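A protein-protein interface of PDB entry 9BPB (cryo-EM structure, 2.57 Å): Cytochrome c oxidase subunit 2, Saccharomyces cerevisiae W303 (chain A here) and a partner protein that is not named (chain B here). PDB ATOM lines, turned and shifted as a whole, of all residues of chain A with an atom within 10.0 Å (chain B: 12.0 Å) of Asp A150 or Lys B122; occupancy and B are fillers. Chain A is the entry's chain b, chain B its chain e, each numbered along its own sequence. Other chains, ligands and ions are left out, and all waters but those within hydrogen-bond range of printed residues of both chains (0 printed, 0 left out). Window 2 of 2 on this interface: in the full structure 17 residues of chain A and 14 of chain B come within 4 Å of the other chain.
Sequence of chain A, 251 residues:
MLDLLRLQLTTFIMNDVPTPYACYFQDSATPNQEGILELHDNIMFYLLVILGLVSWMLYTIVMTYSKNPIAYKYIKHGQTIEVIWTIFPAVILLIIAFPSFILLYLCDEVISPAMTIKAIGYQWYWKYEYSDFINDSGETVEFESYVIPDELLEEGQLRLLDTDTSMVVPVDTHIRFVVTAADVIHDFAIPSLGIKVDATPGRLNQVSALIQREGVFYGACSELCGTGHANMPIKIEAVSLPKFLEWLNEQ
The backbone carbonyl oxygen of Gln A157 lies within hydrogen-bond range of the indole nitrogen of Trp B128, at 2.5 Å. OE1 of Glu A155 lies within salt-bridge range of NZ of Lys B131, 2.8 Å away. The side-chain carboxylate (OE2) of Glu A155 sits close to the side-chain carboxylate (OE1) of Glu B127, at 2.9 Å. The side-chain amino group (NZ) of Lys B122 is in hydrogen-bond range of the backbone carbonyl oxygen (O) of Asp A150, at 2.7 Å.
NH2 of Arg A159 lies within salt-bridge range of OD2 of Asp A150. O of Trp B128 lies within hydrogen-bond range of OG of Ser B132. O of Lys B122 is in hydrogen-bond range of ND2 of Asn B125.
Lys B122 touches Leu A153 (NZ to CB, 3.7 Å). CD2 of Leu A153 touches CG2 of Thr B123 (3.99 Å). Leu A153 touches Trp B128 (O to CH2, 3.3 Å). Trp B128 touches Glu A154. Glu A155 touches Trp B128. N of Gly A156 touches CE2 of Trp B128 (3.5 Å). CE of Lys B131 touches CA of Gly A156 (3.9 Å).
No residue of chain B comes within 4 Å of Pro A149. Of chain B, only Lys B122 (2.7 Å) comes within 4 Å of Asp A150. No residue of chain B comes within 4 Å of Leu A152. Of the printed residues of chain B, Leu A153 touches Lys B122, Thr B123 and Trp B128. Printed residues of chain A within 4 Å of Lys B131: Glu A155 and Gly A156. The nearest residue of chain A that does not touch Lys B122 is Glu A151 (4.8 Å). The nearest printed residue of chain B that does not touch Gln A157 is Ser B132 (4.5 Å).
Hydrophobic or aromatic side chains of chain A within 4 Å of the printed part of chain B: Leu A153. Of the 18 printed residues of chain B, 5 touch a printed residue of chain A. Hydrophobic or aromatic side chains of chain B within 4 Å of the printed part of chain A: Trp B128. Among the printed residues, 11 pairs touch across the chains.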
ATOM      1  N   VAL A 147     -43.308  16.070   3.663  1.00  0.00           N
ATOM      2  CA  VAL A 147     -41.898  16.279   3.371  1.00  0.00           C
ATOM      3  C   VAL A 147     -41.748  17.529   2.511  1.00  0.00           C
ATOM      4  O   VAL A 147     -42.688  17.964   1.833  1.00  0.00           O
ATOM      5  CB  VAL A 147     -41.294  15.045   2.675  1.00  0.00           C
ATOM      6  CG1 VAL A 147     -41.742  14.976   1.224  1.00  0.00           C
ATOM      7  CG2 VAL A 147     -39.774  15.044   2.783  1.00  0.00           C
ATOM      8  N   ILE A 148     -40.562  18.125   2.550  1.00  0.00           N
ATOM      9  CA  ILE A 148     -40.249  19.300   1.744  1.00  0.00           C
ATOM     10  C   ILE A 148     -39.680  18.815   0.414  1.00  0.00           C
ATOM     11  O   ILE A 148     -38.676  18.085   0.417  1.00  0.00           O
ATOM     12  CB  ILE A 148     -39.261  20.227   2.458  1.00  0.00           C
ATOM     13  CG1 ILE A 148     -39.788  20.601   3.842  1.00  0.00           C
ATOM     14  CG2 ILE A 148     -39.021  21.479   1.637  1.00  0.00           C
ATOM     15  CD1 ILE A 148     -38.766  21.282   4.714  1.00  0.00           C
ATOM     16  N   PRO A 149     -40.276  19.176  -0.719  1.00  0.00           N
ATOM     17  CA  PRO A 149     -39.771  18.692  -2.006  1.00  0.00           C
ATOM     18  C   PRO A 149     -38.419  19.302  -2.341  1.00  0.00           C
ATOM     19  O   PRO A 149     -37.994  20.306  -1.767  1.00  0.00           O
ATOM     20  CB  PRO A 149     -40.843  19.138  -3.007  1.00  0.00           C
ATOM     21  CG  PRO A 149     -42.030  19.540  -2.174  1.00  0.00           C
ATOM     22  CD  PRO A 149     -41.474  20.014  -0.876  1.00  0.00           C
ATOM     23  N   ASP A 150     -37.735  18.666  -3.295  1.00  0.00           N
ATOM     24  CA  ASP A 150     -36.416  19.143  -3.696  1.00  0.00           C
ATOM     25  C   ASP A 150     -36.490  20.483  -4.414  1.00  0.00           C
ATOM     26  O   ASP A 150     -35.508  21.234  -4.421  1.00  0.00           O
ATOM     27  CB  ASP A 150     -35.727  18.104  -4.581  1.00  0.00           C
ATOM     28  CG  ASP A 150     -35.304  16.871  -3.808  1.00  0.00           C
ATOM     29  OD1 ASP A 150     -35.558  16.818  -2.587  1.00  0.00           O
ATOM     30  OD2 ASP A 150     -34.711  15.959  -4.419  1.00  0.00           O
ATOM     31  N   GLU A 151     -37.631  20.801  -5.028  1.00  0.00           N
ATOM     32  CA  GLU A 151     -37.768  22.090  -5.697  1.00  0.00           C
ATOM     33  C   GLU A 151     -37.709  23.239  -4.699  1.00  0.00           C
ATOM     34  O   GLU A 151     -37.129  24.292  -4.988  1.00  0.00           O
ATOM     35  CB  GLU A 151     -39.071  22.139  -6.493  1.00  0.00           C
ATOM     36  CG  GLU A 151     -39.234  23.402  -7.330  1.00  0.00           C
ATOM     37  CD  GLU A 151     -40.471  23.369  -8.205  1.00  0.00           C
ATOM     38  OE1 GLU A 151     -41.244  22.395  -8.108  1.00  0.00           O
ATOM     39  OE2 GLU A 151     -40.667  24.317  -8.993  1.00  0.00           O
ATOM     40  N   LEU A 152     -38.301  23.056  -3.519  1.00  0.00           N
ATOM     41  CA  LEU A 152     -38.355  24.090  -2.494  1.00  0.00           C
ATOM     42  C   LEU A 152     -37.425  23.804  -1.323  1.00  0.00           C
ATOM     43  O   LEU A 152     -37.634  24.339  -0.229  1.00  0.00           O
ATOM     44  CB  LEU A 152     -39.789  24.264  -1.995  1.00  0.00           C
ATOM     45  CG  LEU A 152     -40.896  24.194  -3.047  1.00  0.00           C
ATOM     46  CD1 LEU A 152     -42.258  24.208  -2.379  1.00  0.00           C
ATOM     47  CD2 LEU A 152     -40.770  25.342  -4.033  1.00  0.00           C
ATOM     48  N   LEU A 153     -36.406  22.973  -1.526  1.00  0.00           N
ATOM     49  CA  LEU A 153     -35.470  22.638  -0.457  1.00  0.00           C
ATOM     50  C   LEU A 153     -34.611  23.858  -0.140  1.00  0.00           C
ATOM     51  O   LEU A 153     -33.654  24.157  -0.859  1.00  0.00           O
ATOM     52  CB  LEU A 153     -34.608  21.449  -0.869  1.00  0.00           C
ATOM     53  CG  LEU A 153     -34.181  20.482   0.236  1.00  0.00           C
ATOM     54  CD1 LEU A 153     -35.361  20.109   1.114  1.00  0.00           C
ATOM     55  CD2 LEU A 153     -33.553  19.239  -0.368  1.00  0.00           C
ATOM     56  N   GLU A 154     -34.956  24.560   0.938  1.00  0.00           N
ATOM     57  CA  GLU A 154     -34.282  25.803   1.286  1.00  0.00           C
ATOM     58  C   GLU A 154     -32.820  25.543   1.631  1.00  0.00           C
ATOM     59  O   GLU A 154     -32.454  24.467   2.110  1.00  0.00           O
ATOM     60  CB  GLU A 154     -34.994  26.478   2.458  1.00  0.00           C
ATOM     61  CG  GLU A 154     -34.570  27.916   2.721  1.00  0.00           C
ATOM     62  CD  GLU A 154     -33.510  28.030   3.799  1.00  0.00           C
ATOM     63  OE1 GLU A 154     -33.347  27.070   4.582  1.00  0.00           O
ATOM     64  OE2 GLU A 154     -32.842  29.082   3.867  1.00  0.00           O
ATOM     65  N   GLU A 155     -31.984  26.550   1.385  1.00  0.00           N
ATOM     66  CA  GLU A 155     -30.537  26.400   1.475  1.00  0.00           C
ATOM     67  C   GLU A 155     -30.083  26.121   2.904  1.00  0.00           C
ATOM     68  O   GLU A 155     -30.081  27.020   3.751  1.00  0.00           O
ATOM     69  CB  GLU A 155     -29.851  27.655   0.927  1.00  0.00           C
ATOM     70  CG  GLU A 155     -28.397  27.461   0.534  1.00  0.00           C
ATOM     71  CD  GLU A 155     -27.439  27.870   1.632  1.00  0.00           C
ATOM     72  OE1 GLU A 155     -27.811  28.737   2.449  1.00  0.00           O
ATOM     73  OE2 GLU A 155     -26.314  27.327   1.673  1.00  0.00           O
ATOM     74  N   GLY A 156     -29.695  24.878   3.175  1.00  0.00           N
ATOM     75  CA  GLY A 156     -29.232  24.464   4.489  1.00  0.00           C
ATOM     76  C   GLY A 156     -30.045  23.366   5.144  1.00  0.00           C
ATOM     77  O   GLY A 156     -29.734  22.984   6.281  1.00  0.00           O
ATOM     78  N   GLN A 157     -31.072  22.835   4.486  1.00  0.00           N
ATOM     79  CA  GLN A 157     -31.952  21.846   5.088  1.00  0.00           C
ATOM     80  C   GLN A 157     -31.481  20.426   4.785  1.00  0.00           C
ATOM     81  O   GLN A 157     -30.665  20.187   3.893  1.00  0.00           O
ATOM     82  CB  GLN A 157     -33.386  22.039   4.597  1.00  0.00           C
ATOM     83  CG  GLN A 157     -34.014  23.352   5.036  1.00  0.00           C
ATOM     84  CD  GLN A 157     -35.434  23.512   4.540  1.00  0.00           C
ATOM     85  OE1 GLN A 157     -35.930  22.683   3.781  1.00  0.00           O
ATOM     86  NE2 GLN A 157     -36.099  24.574   4.976  1.00  0.00           N
ATOM     87  N   LEU A 158     -32.014  19.477   5.552  1.00  0.00           N
ATOM     88  CA  LEU A 158     -31.638  18.074   5.416  1.00  0.00           C
ATOM     89  C   LEU A 158     -32.557  17.375   4.424  1.00  0.00           C
ATOM     90  O   LEU A 158     -33.781  17.518   4.490  1.00  0.00           O
ATOM     91  CB  LEU A 158     -31.689  17.371   6.772  1.00  0.00           C
ATOM     92  CG  LEU A 158     -30.562  17.683   7.759  1.00  0.00           C
ATOM     93  CD1 LEU A 158     -30.857  18.942   8.562  1.00  0.00           C
ATOM     94  CD2 LEU A 158     -30.329  16.500   8.674  1.00  0.00           C
ATOM     95  N   ARG A 159     -31.966  16.613   3.508  1.00  0.00           N
ATOM     96  CA  ARG A 159     -32.732  15.989   2.440  1.00  0.00           C
ATOM     97  C   ARG A 159     -33.433  14.724   2.928  1.00  0.00           C
ATOM     98  O   ARG A 159     -32.861  13.910   3.655  1.00  0.00           O
ATOM     99  CB  ARG A 159     -31.818  15.659   1.264  1.00  0.00           C
ATOM    100  CG  ARG A 159     -32.548  15.171   0.036  1.00  0.00           C
ATOM    101  CD  ARG A 159     -31.583  14.859  -1.088  1.00  0.00           C
ATOM    102  NE  ARG A 159     -32.291  14.514  -2.313  1.00  0.00           N
ATOM    103  CZ  ARG A 159     -32.710  13.292  -2.608  1.00  0.00           C
ATOM    104  NH1 ARG A 159     -32.507  12.276  -1.789  1.00  0.00           N
ATOM    105  NH2 ARG A 159     -33.357  13.089  -3.752  1.00  0.00           N
ATOM    106  N   LEU A 160     -34.691  14.567   2.511  1.00  0.00           N
ATOM    107  CA  LEU A 160     -35.544  13.431   2.867  1.00  0.00           C
ATOM    108  C   LEU A 160     -35.724  13.275   4.370  1.00  0.00           C
ATOM    109  O   LEU A 160     -36.120  12.206   4.838  1.00  0.00           O
ATOM    110  CB  LEU A 160     -35.019  12.113   2.288  1.00  0.00           C
ATOM    111  CG  LEU A 160     -35.007  11.917   0.778  1.00  0.00           C
ATOM    112  CD1 LEU A 160     -34.324  10.608   0.477  1.00  0.00           C
ATOM    113  CD2 LEU A 160     -36.415  11.926   0.230  1.00  0.00           C
ATOM    114  N   LEU A 161     -35.442  14.313   5.146  1.00  0.00           N
ATOM    115  CA  LEU A 161     -35.511  14.209   6.593  1.00  0.00           C
ATOM    116  C   LEU A 161     -36.258  15.352   7.250  1.00  0.00           C
ATOM    117  O   LEU A 161     -36.772  15.167   8.358  1.00  0.00           O
ATOM    118  CB  LEU A 161     -34.099  14.132   7.187  1.00  0.00           C
ATOM    119  CG  LEU A 161     -33.929  13.533   8.580  1.00  0.00           C
ATOM    120  CD1 LEU A 161     -34.624  12.189   8.645  1.00  0.00           C
ATOM    121  CD2 LEU A 161     -32.456  13.392   8.909  1.00  0.00           C
ATOM    122  N   ASP A 162     -36.367  16.507   6.603  1.00  0.00           N
ATOM    123  CA  ASP A 162     -36.941  17.696   7.210  1.00  0.00           C
ATOM    124  C   ASP A 162     -38.312  17.959   6.604  1.00  0.00           C
ATOM    125  O   ASP A 162     -38.476  17.893   5.381  1.00  0.00           O
ATOM    126  CB  ASP A 162     -36.020  18.901   7.006  1.00  0.00           C
ATOM    127  CG  ASP A 162     -36.206  19.961   8.066  1.00  0.00           C
ATOM    128  OD1 ASP A 162     -35.748  19.742   9.207  1.00  0.00           O
ATOM    129  OD2 ASP A 162     -36.809  21.012   7.763  1.00  0.00           O
ATOM    130  N   ALA A 230     -40.798   6.529   1.029  1.00  0.00           N
ATOM    131  CA  ALA A 230     -39.584   7.259   1.363  1.00  0.00           C
ATOM    132  C   ALA A 230     -39.863   8.688   1.806  1.00  0.00           C
ATOM    133  O   ALA A 230     -39.061   9.259   2.551  1.00  0.00           O
ATOM    134  CB  ALA A 230     -38.629   7.261   0.173  1.00  0.00           C
ATOM    135  N   ASN A 231     -40.972   9.278   1.367  1.00  0.00           N
ATOM    136  CA  ASN A 231     -41.291  10.670   1.682  1.00  0.00           C
ATOM    137  C   ASN A 231     -42.221  10.762   2.892  1.00  0.00           C
ATOM    138  O   ASN A 231     -43.302  11.346   2.832  1.00  0.00           O
ATOM    139  CB  ASN A 231     -41.909  11.349   0.463  1.00  0.00           C
ATOM    140  CG  ASN A 231     -40.922  11.510  -0.676  1.00  0.00           C
ATOM    141  OD1 ASN A 231     -39.780  11.915  -0.473  1.00  0.00           O
ATOM    142  ND2 ASN A 231     -41.363  11.193  -1.887  1.00  0.00           N
ATOM    143  N   GLY B 118     -27.196   9.838 -13.659  1.00  0.00           N
ATOM    144  CA  GLY B 118     -27.701  11.177 -13.456  1.00  0.00           C
ATOM    145  C   GLY B 118     -26.775  12.035 -12.616  1.00  0.00           C
ATOM    146  O   GLY B 118     -25.790  11.573 -12.041  1.00  0.00           O
ATOM    147  N   GLN B 119     -27.111  13.320 -12.549  1.00  0.00           N
ATOM    148  CA  GLN B 119     -26.317  14.264 -11.782  1.00  0.00           C
ATOM    149  C   GLN B 119     -26.532  14.057 -10.285  1.00  0.00           C
ATOM    150  O   GLN B 119     -27.515  13.457  -9.845  1.00  0.00           O
ATOM    151  CB  GLN B 119     -26.662  15.702 -12.173  1.00  0.00           C
ATOM    152  CG  GLN B 119     -26.533  15.989 -13.660  1.00  0.00           C
ATOM    153  CD  GLN B 119     -25.328  15.309 -14.286  1.00  0.00           C
ATOM    154  OE1 GLN B 119     -24.184  15.600 -13.937  1.00  0.00           O
ATOM    155  NE2 GLN B 119     -25.582  14.395 -15.216  1.00  0.00           N
ATOM    156  N   ASP B 120     -25.588  14.567  -9.502  1.00  0.00           N
ATOM    157  CA  ASP B 120     -25.659  14.439  -8.056  1.00  0.00           C
ATOM    158  C   ASP B 120     -26.739  15.354  -7.488  1.00  0.00           C
ATOM    159  O   ASP B 120     -27.192  16.305  -8.132  1.00  0.00           O
ATOM    160  CB  ASP B 120     -24.310  14.772  -7.421  1.00  0.00           C
ATOM    161  CG  ASP B 120     -23.756  16.102  -7.893  1.00  0.00           C
ATOM    162  OD1 ASP B 120     -23.654  16.304  -9.121  1.00  0.00           O
ATOM    163  OD2 ASP B 120     -23.423  16.946  -7.034  1.00  0.00           O
ATOM    164  N   ALA B 121     -27.156  15.046  -6.264  1.00  0.00           N
ATOM    165  CA  ALA B 121     -28.092  15.909  -5.559  1.00  0.00           C
ATOM    166  C   ALA B 121     -27.443  17.253  -5.256  1.00  0.00           C
ATOM    167  O   ALA B 121     -26.230  17.354  -5.062  1.00  0.00           O
ATOM    168  CB  ALA B 121     -28.564  15.244  -4.266  1.00  0.00           C
ATOM    169  N   LYS B 122     -28.270  18.299  -5.221  1.00  0.00           N
ATOM    170  CA  LYS B 122     -27.762  19.647  -5.000  1.00  0.00           C
ATOM    171  C   LYS B 122     -27.335  19.893  -3.558  1.00  0.00           C
ATOM    172  O   LYS B 122     -26.839  20.982  -3.258  1.00  0.00           O
ATOM    173  CB  LYS B 122     -28.818  20.676  -5.411  1.00  0.00           C
ATOM    174  CG  LYS B 122     -30.050  20.691  -4.525  1.00  0.00           C
ATOM    175  CD  LYS B 122     -31.128  21.592  -5.098  1.00  0.00           C
ATOM    176  CE  LYS B 122     -32.315  21.691  -4.160  1.00  0.00           C
ATOM    177  NZ  LYS B 122     -32.984  20.375  -3.987  1.00  0.00           N
ATOM    178  N   THR B 123     -27.511  18.919  -2.670  1.00  0.00           N
ATOM    179  CA  THR B 123     -27.174  19.074  -1.260  1.00  0.00           C
ATOM    180  C   THR B 123     -25.798  18.521  -0.903  1.00  0.00           C
ATOM    181  O   THR B 123     -25.436  18.523   0.277  1.00  0.00           O
ATOM    182  CB  THR B 123     -28.238  18.395  -0.391  1.00  0.00           C
ATOM    183  OG1 THR B 123     -28.077  16.973  -0.455  1.00  0.00           O
ATOM    184  CG2 THR B 123     -29.630  18.758  -0.879  1.00  0.00           C
ATOM    185  N   MET B 124     -25.023  18.053  -1.884  1.00  0.00           N
ATOM    186  CA  MET B 124     -23.706  17.470  -1.650  1.00  0.00           C
ATOM    187  C   MET B 124     -22.571  18.440  -1.977  1.00  0.00           C
ATOM    188  O   MET B 124     -21.518  18.017  -2.466  1.00  0.00           O
ATOM    189  CB  MET B 124     -23.552  16.183  -2.462  1.00  0.00           C
ATOM    190  CG  MET B 124     -24.550  15.091  -2.109  1.00  0.00           C
ATOM    191  SD  MET B 124     -24.287  14.390  -0.470  1.00  0.00           S
ATOM    192  CE  MET B 124     -23.575  12.807  -0.898  1.00  0.00           C
ATOM    193  N   ASN B 125     -22.762  19.731  -1.707  1.00  0.00           N
ATOM    194  CA  ASN B 125     -21.847  20.773  -2.158  1.00  0.00           C
ATOM    195  C   ASN B 125     -20.731  21.091  -1.172  1.00  0.00           C
ATOM    196  O   ASN B 125     -19.851  21.892  -1.508  1.00  0.00           O
ATOM    197  CB  ASN B 125     -22.631  22.057  -2.445  1.00  0.00           C
ATOM    198  CG  ASN B 125     -23.834  21.817  -3.326  1.00  0.00           C
ATOM    199  OD1 ASN B 125     -23.993  20.736  -3.893  1.00  0.00           O
ATOM    200  ND2 ASN B 125     -24.694  22.820  -3.441  1.00  0.00           N
ATOM    201  N   LYS B 126     -20.771  20.522   0.036  1.00  0.00           N
ATOM    202  CA  LYS B 126     -19.830  20.764   1.130  1.00  0.00           C
ATOM    203  C   LYS B 126     -20.052  22.142   1.746  1.00  0.00           C
ATOM    204  O   LYS B 126     -19.521  22.442   2.818  1.00  0.00           O
ATOM    205  CB  LYS B 126     -18.375  20.612   0.666  1.00  0.00           C
ATOM    206  CG  LYS B 126     -17.357  20.480   1.796  1.00  0.00           C
ATOM    207  CD  LYS B 126     -16.617  21.782   2.067  1.00  0.00           C
ATOM    208  CE  LYS B 126     -15.610  21.613   3.193  1.00  0.00           C
ATOM    209  NZ  LYS B 126     -14.901  22.883   3.506  1.00  0.00           N
ATOM    210  N   GLU B 127     -20.876  22.968   1.108  1.00  0.00           N
ATOM    211  CA  GLU B 127     -21.360  24.192   1.728  1.00  0.00           C
ATOM    212  C   GLU B 127     -22.779  24.039   2.246  1.00  0.00           C
ATOM    213  O   GLU B 127     -23.154  24.703   3.217  1.00  0.00           O
ATOM    214  CB  GLU B 127     -21.284  25.367   0.741  1.00  0.00           C
ATOM    215  CG  GLU B 127     -22.252  25.303  -0.432  1.00  0.00           C
ATOM    216  CD  GLU B 127     -23.562  26.016  -0.146  1.00  0.00           C
ATOM    217  OE1 GLU B 127     -23.612  26.797   0.827  1.00  0.00           O
ATOM    218  OE2 GLU B 127     -24.538  25.802  -0.894  1.00  0.00           O
ATOM    219  N   TRP B 128     -23.567  23.173   1.606  1.00  0.00           N
ATOM    220  CA  TRP B 128     -24.806  22.701   2.207  1.00  0.00           C
ATOM    221  C   TRP B 128     -24.520  21.881   3.457  1.00  0.00           C
ATOM    222  O   TRP B 128     -25.191  22.041   4.482  1.00  0.00           O
ATOM    223  CB  TRP B 128     -25.578  21.871   1.182  1.00  0.00           C
ATOM    224  CG  TRP B 128     -27.046  21.770   1.428  1.00  0.00           C
ATOM    225  CD1 TRP B 128     -27.670  21.037   2.394  1.00  0.00           C
ATOM    226  CD2 TRP B 128     -28.085  22.412   0.677  1.00  0.00           C
ATOM    227  NE1 TRP B 128     -29.030  21.189   2.297  1.00  0.00           N
ATOM    228  CE2 TRP B 128     -29.311  22.028   1.250  1.00  0.00           C
ATOM    229  CE3 TRP B 128     -28.095  23.277  -0.420  1.00  0.00           C
ATOM    230  CZ2 TRP B 128     -30.534  22.478   0.763  1.00  0.00           C
ATOM    231  CZ3 TRP B 128     -29.310  23.722  -0.901  1.00  0.00           C
ATOM    232  CH2 TRP B 128     -30.512  23.323  -0.311  1.00  0.00           C
ATOM    233  N   GLN B 129     -23.510  21.008   3.392  1.00  0.00           N
ATOM    234  CA  GLN B 129     -23.193  20.137   4.520  1.00  0.00           C
ATOM    235  C   GLN B 129     -22.589  20.921   5.679  1.00  0.00           C
ATOM    236  O   GLN B 129     -22.802  20.576   6.847  1.00  0.00           O
ATOM    237  CB  GLN B 129     -22.251  19.023   4.066  1.00  0.00           C
ATOM    238  CG  GLN B 129     -22.865  18.078   3.043  1.00  0.00           C
ATOM    239  CD  GLN B 129     -21.878  17.054   2.520  1.00  0.00           C
ATOM    240  OE1 GLN B 129     -20.686  17.117   2.810  1.00  0.00           O
ATOM    241  NE2 GLN B 129     -22.373  16.099   1.741  1.00  0.00           N
ATOM    242  N   LEU B 130     -21.822  21.972   5.380  1.00  0.00           N
ATOM    243  CA  LEU B 130     -21.329  22.844   6.440  1.00  0.00           C
ATOM    244  C   LEU B 130     -22.469  23.628   7.080  1.00  0.00           C
ATOM    245  O   LEU B 130     -22.446  23.893   8.287  1.00  0.00           O
ATOM    246  CB  LEU B 130     -20.269  23.800   5.891  1.00  0.00           C
ATOM    247  CG  LEU B 130     -18.800  23.428   6.102  1.00  0.00           C
ATOM    248  CD1 LEU B 130     -17.898  24.559   5.643  1.00  0.00           C
ATOM    249  CD2 LEU B 130     -18.535  23.090   7.559  1.00  0.00           C
ATOM    250  N   LYS B 131     -23.470  24.013   6.285  1.00  0.00           N
ATOM    251  CA  LYS B 131     -24.601  24.759   6.827  1.00  0.00           C
ATOM    252  C   LYS B 131     -25.555  23.860   7.604  1.00  0.00           C
ATOM    253  O   LYS B 131     -26.310  24.350   8.450  1.00  0.00           O
ATOM    254  CB  LYS B 131     -25.346  25.475   5.704  1.00  0.00           C
ATOM    255  CG  LYS B 131     -24.948  26.927   5.533  1.00  0.00           C
ATOM    256  CD  LYS B 131     -26.065  27.723   4.896  1.00  0.00           C
ATOM    257  CE  LYS B 131     -27.333  27.659   5.732  1.00  0.00           C
ATOM    258  NZ  LYS B 131     -28.381  28.578   5.211  1.00  0.00           N
ATOM    259  N   SER B 132     -25.545  22.555   7.328  1.00  0.00           N
ATOM    260  CA  SER B 132     -26.389  21.636   8.084  1.00  0.00           C
ATOM    261  C   SER B 132     -25.963  21.560   9.546  1.00  0.00           C
ATOM    262  O   SER B 132     -26.785  21.254  10.416  1.00  0.00           O
ATOM    263  CB  SER B 132     -26.355  20.245   7.451  1.00  0.00           C
ATOM    264  OG  SER B 132     -26.754  20.282   6.093  1.00  0.00           O
ATOM    265  N   GLN B 149     -21.855  15.744   9.714  1.00  0.00           N
ATOM    266  CA  GLN B 149     -22.626  15.803   8.468  1.00  0.00           C
ATOM    267  C   GLN B 149     -21.772  16.198   7.264  1.00  0.00           C
ATOM    268  O   GLN B 149     -22.291  16.715   6.273  1.00  0.00           O
ATOM    269  CB  GLN B 149     -23.815  16.762   8.599  1.00  0.00           C
ATOM    270  CG  GLN B 149     -25.067  16.144   9.194  1.00  0.00           C
ATOM    271  CD  GLN B 149     -25.387  14.791   8.600  1.00  0.00           C
ATOM    272  OE1 GLN B 149     -25.481  13.797   9.315  1.00  0.00           O
ATOM    273  NE2 GLN B 149     -25.562  14.745   7.285  1.00  0.00           N
ATOM    274  N   GLN B 151     -19.158  14.860   4.369  1.00  0.00           N
ATOM    275  CA  GLN B 151     -18.622  13.683   3.694  1.00  0.00           C
ATOM    276  C   GLN B 151     -18.138  13.991   2.281  1.00  0.00           C
ATOM    277  O   GLN B 151     -17.908  13.056   1.502  1.00  0.00           O
ATOM    278  CB  GLN B 151     -19.673  12.575   3.638  1.00  0.00           C
ATOM    279  CG  GLN B 151     -21.022  13.049   3.140  1.00  0.00           C
ATOM    280  CD  GLN B 151     -22.005  11.918   2.952  1.00  0.00           C
ATOM    281  OE1 GLN B 151     -21.627  10.748   2.943  1.00  0.00           O
ATOM    282  NE2 GLN B 151     -23.278  12.260   2.800  1.00  0.00           N
ATOM    283  N   SER B 152     -17.988  15.266   1.930  1.00  0.00           N
ATOM    284  CA  SER B 152     -17.667  15.686   0.565  1.00  0.00           C
ATOM    285  C   SER B 152     -16.460  14.968  -0.034  1.00  0.00           C
ATOM    286  O   SER B 152     -16.200  15.073  -1.234  1.00  0.00           O
ATOM    287  CB  SER B 152     -17.422  17.193   0.529  1.00  0.00           C
ATOM    288  OG  SER B 152     -16.978  17.610  -0.749  1.00  0.00           O
